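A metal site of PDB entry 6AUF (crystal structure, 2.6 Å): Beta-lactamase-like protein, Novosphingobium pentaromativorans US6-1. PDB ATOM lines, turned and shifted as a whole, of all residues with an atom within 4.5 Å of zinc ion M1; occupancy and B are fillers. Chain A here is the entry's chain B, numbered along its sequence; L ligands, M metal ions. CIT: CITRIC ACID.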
ATOM      1  N   HIS A 107      -7.557 -20.912  20.200  1.00  0.00           N
ATOM      2  CA  HIS A 107      -6.401 -20.891  19.314  1.00  0.00           C
ATOM      3  C   HIS A 107      -6.656 -21.860  18.160  1.00  0.00           C
ATOM      4  O   HIS A 107      -7.676 -22.546  18.118  1.00  0.00           O
ATOM      5  CB  HIS A 107      -5.092 -21.166  20.066  1.00  0.00           C
ATOM      6  CG  HIS A 107      -4.866 -22.600  20.442  1.00  0.00           C
ATOM      7  ND1 HIS A 107      -5.036 -23.064  21.730  1.00  0.00           N
ATOM      8  CD2 HIS A 107      -4.407 -23.642  19.721  1.00  0.00           C
ATOM      9  CE1 HIS A 107      -4.701 -24.352  21.776  1.00  0.00           C
ATOM     10  NE2 HIS A 107      -4.334 -24.725  20.567  1.00  0.00           N
ATOM     11  N   HIS A 109      -5.685 -24.623  16.538  1.00  0.00           N
ATOM     12  CA  HIS A 109      -5.327 -26.027  16.364  1.00  0.00           C
ATOM     13  C   HIS A 109      -6.577 -26.872  16.205  1.00  0.00           C
ATOM     14  O   HIS A 109      -7.663 -26.489  16.645  1.00  0.00           O
ATOM     15  CB  HIS A 109      -4.488 -26.505  17.548  1.00  0.00           C
ATOM     16  CG  HIS A 109      -3.122 -25.891  17.578  1.00  0.00           C
ATOM     17  ND1 HIS A 109      -2.365 -25.802  18.725  1.00  0.00           N
ATOM     18  CD2 HIS A 109      -2.363 -25.332  16.594  1.00  0.00           C
ATOM     19  CE1 HIS A 109      -1.206 -25.230  18.453  1.00  0.00           C
ATOM     20  NE2 HIS A 109      -1.183 -24.936  17.170  1.00  0.00           N
ATOM     21  N   HIS A 112      -9.091 -27.904  19.017  1.00  0.00           N
ATOM     22  CA  HIS A 112      -9.957 -26.891  19.571  1.00  0.00           C
ATOM     23  C   HIS A 112     -10.902 -26.270  18.564  1.00  0.00           C
ATOM     24  O   HIS A 112     -12.014 -25.873  18.932  1.00  0.00           O
ATOM     25  CB  HIS A 112      -9.128 -25.771  20.217  1.00  0.00           C
ATOM     26  CG  HIS A 112      -8.238 -26.258  21.315  1.00  0.00           C
ATOM     27  ND1 HIS A 112      -8.679 -26.411  22.609  1.00  0.00           N
ATOM     28  CD2 HIS A 112      -6.941 -26.634  21.304  1.00  0.00           C
ATOM     29  CE1 HIS A 112      -7.681 -26.855  23.353  1.00  0.00           C
ATOM     30  NE2 HIS A 112      -6.613 -26.994  22.593  1.00  0.00           N
ATOM     31  N   GLN A 148       4.882 -25.726  16.222  1.00  0.00           N
ATOM     32  CA  GLN A 148       4.433 -27.107  16.088  1.00  0.00           C
ATOM     33  C   GLN A 148       4.189 -27.538  14.656  1.00  0.00           C
ATOM     34  O   GLN A 148       4.002 -28.734  14.419  1.00  0.00           O
ATOM     35  CB  GLN A 148       3.151 -27.325  16.884  1.00  0.00           C
ATOM     36  CG  GLN A 148       3.367 -27.489  18.357  1.00  0.00           C
ATOM     37  CD  GLN A 148       2.134 -28.023  19.024  1.00  0.00           C
ATOM     38  OE1 GLN A 148       1.870 -29.234  19.004  1.00  0.00           O
ATOM     39  NE2 GLN A 148       1.337 -27.126  19.597  1.00  0.00           N
ATOM     40  N   HIS A 185       1.058 -19.754  23.253  1.00  0.00           N
ATOM     41  CA  HIS A 185       1.045 -21.152  22.850  1.00  0.00           C
ATOM     42  C   HIS A 185       1.136 -21.304  21.342  1.00  0.00           C
ATOM     43  O   HIS A 185       1.728 -22.283  20.858  1.00  0.00           O
ATOM     44  CB  HIS A 185      -0.210 -21.844  23.409  1.00  0.00           C
ATOM     45  CG  HIS A 185      -0.539 -23.148  22.735  1.00  0.00           C
ATOM     46  ND1 HIS A 185       0.081 -24.343  23.066  1.00  0.00           N
ATOM     47  CD2 HIS A 185      -1.401 -23.444  21.733  1.00  0.00           C
ATOM     48  CE1 HIS A 185      -0.396 -25.313  22.304  1.00  0.00           C
ATOM     49  NE2 HIS A 185      -1.294 -24.795  21.490  1.00  0.00           N
HETATM   50  C1  CIT L   1      -2.445 -27.552  24.487  1.00  0.00           C
HETATM   51  O1  CIT L   1      -2.071 -27.027  25.565  1.00  0.00           O
HETATM   52  O2  CIT L   1      -3.455 -27.084  23.900  1.00  0.00           O
HETATM   53  C2  CIT L   1      -1.662 -28.726  23.907  1.00  0.00           C
HETATM   54  C3  CIT L   1      -1.935 -29.087  22.440  1.00  0.00           C
HETATM   55  O7  CIT L   1      -1.374 -28.213  21.462  1.00  0.00           O
HETATM   56  C4  CIT L   1      -1.473 -30.553  22.335  1.00  0.00           C
HETATM   57  C5  CIT L   1      -1.618 -31.182  20.961  1.00  0.00           C
HETATM   58  O3  CIT L   1      -0.601 -31.672  20.398  1.00  0.00           O
HETATM   59  O4  CIT L   1      -2.725 -31.225  20.364  1.00  0.00           O
HETATM   60  C6  CIT L   1      -3.409 -29.066  22.208  1.00  0.00           C
HETATM   61  O5  CIT L   1      -3.896 -28.108  21.550  1.00  0.00           O
HETATM   62  O6  CIT L   1      -4.109 -29.992  22.666  1.00  0.00           O
HETATM   63 ZN    ZN M   1      -2.707 -26.032  20.588  1.00  0.00          ZN
HETATM   64 ZN    ZN M   2      -5.110 -28.184  22.986  1.00  0.00          ZN
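Zinc ion M1 is bound by a ring nitrogen (ND1) of His 109, a ring nitrogen (NE2) of His 185, a ring nitrogen (NE2) of His 107 and an oxygen (O5) of the ligand.
Zinc ion M1 has four donor atoms within binding distance.
Slightly farther from zinc ion M1 lies O7 of the ligand (2.7 Å).
Three residues have an atom within 4 Å of zinc ion M1: His 107, His 109 and His 185.
Along chain A the residues within 4 Å of zinc ion M1 span positions 107 to 185.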
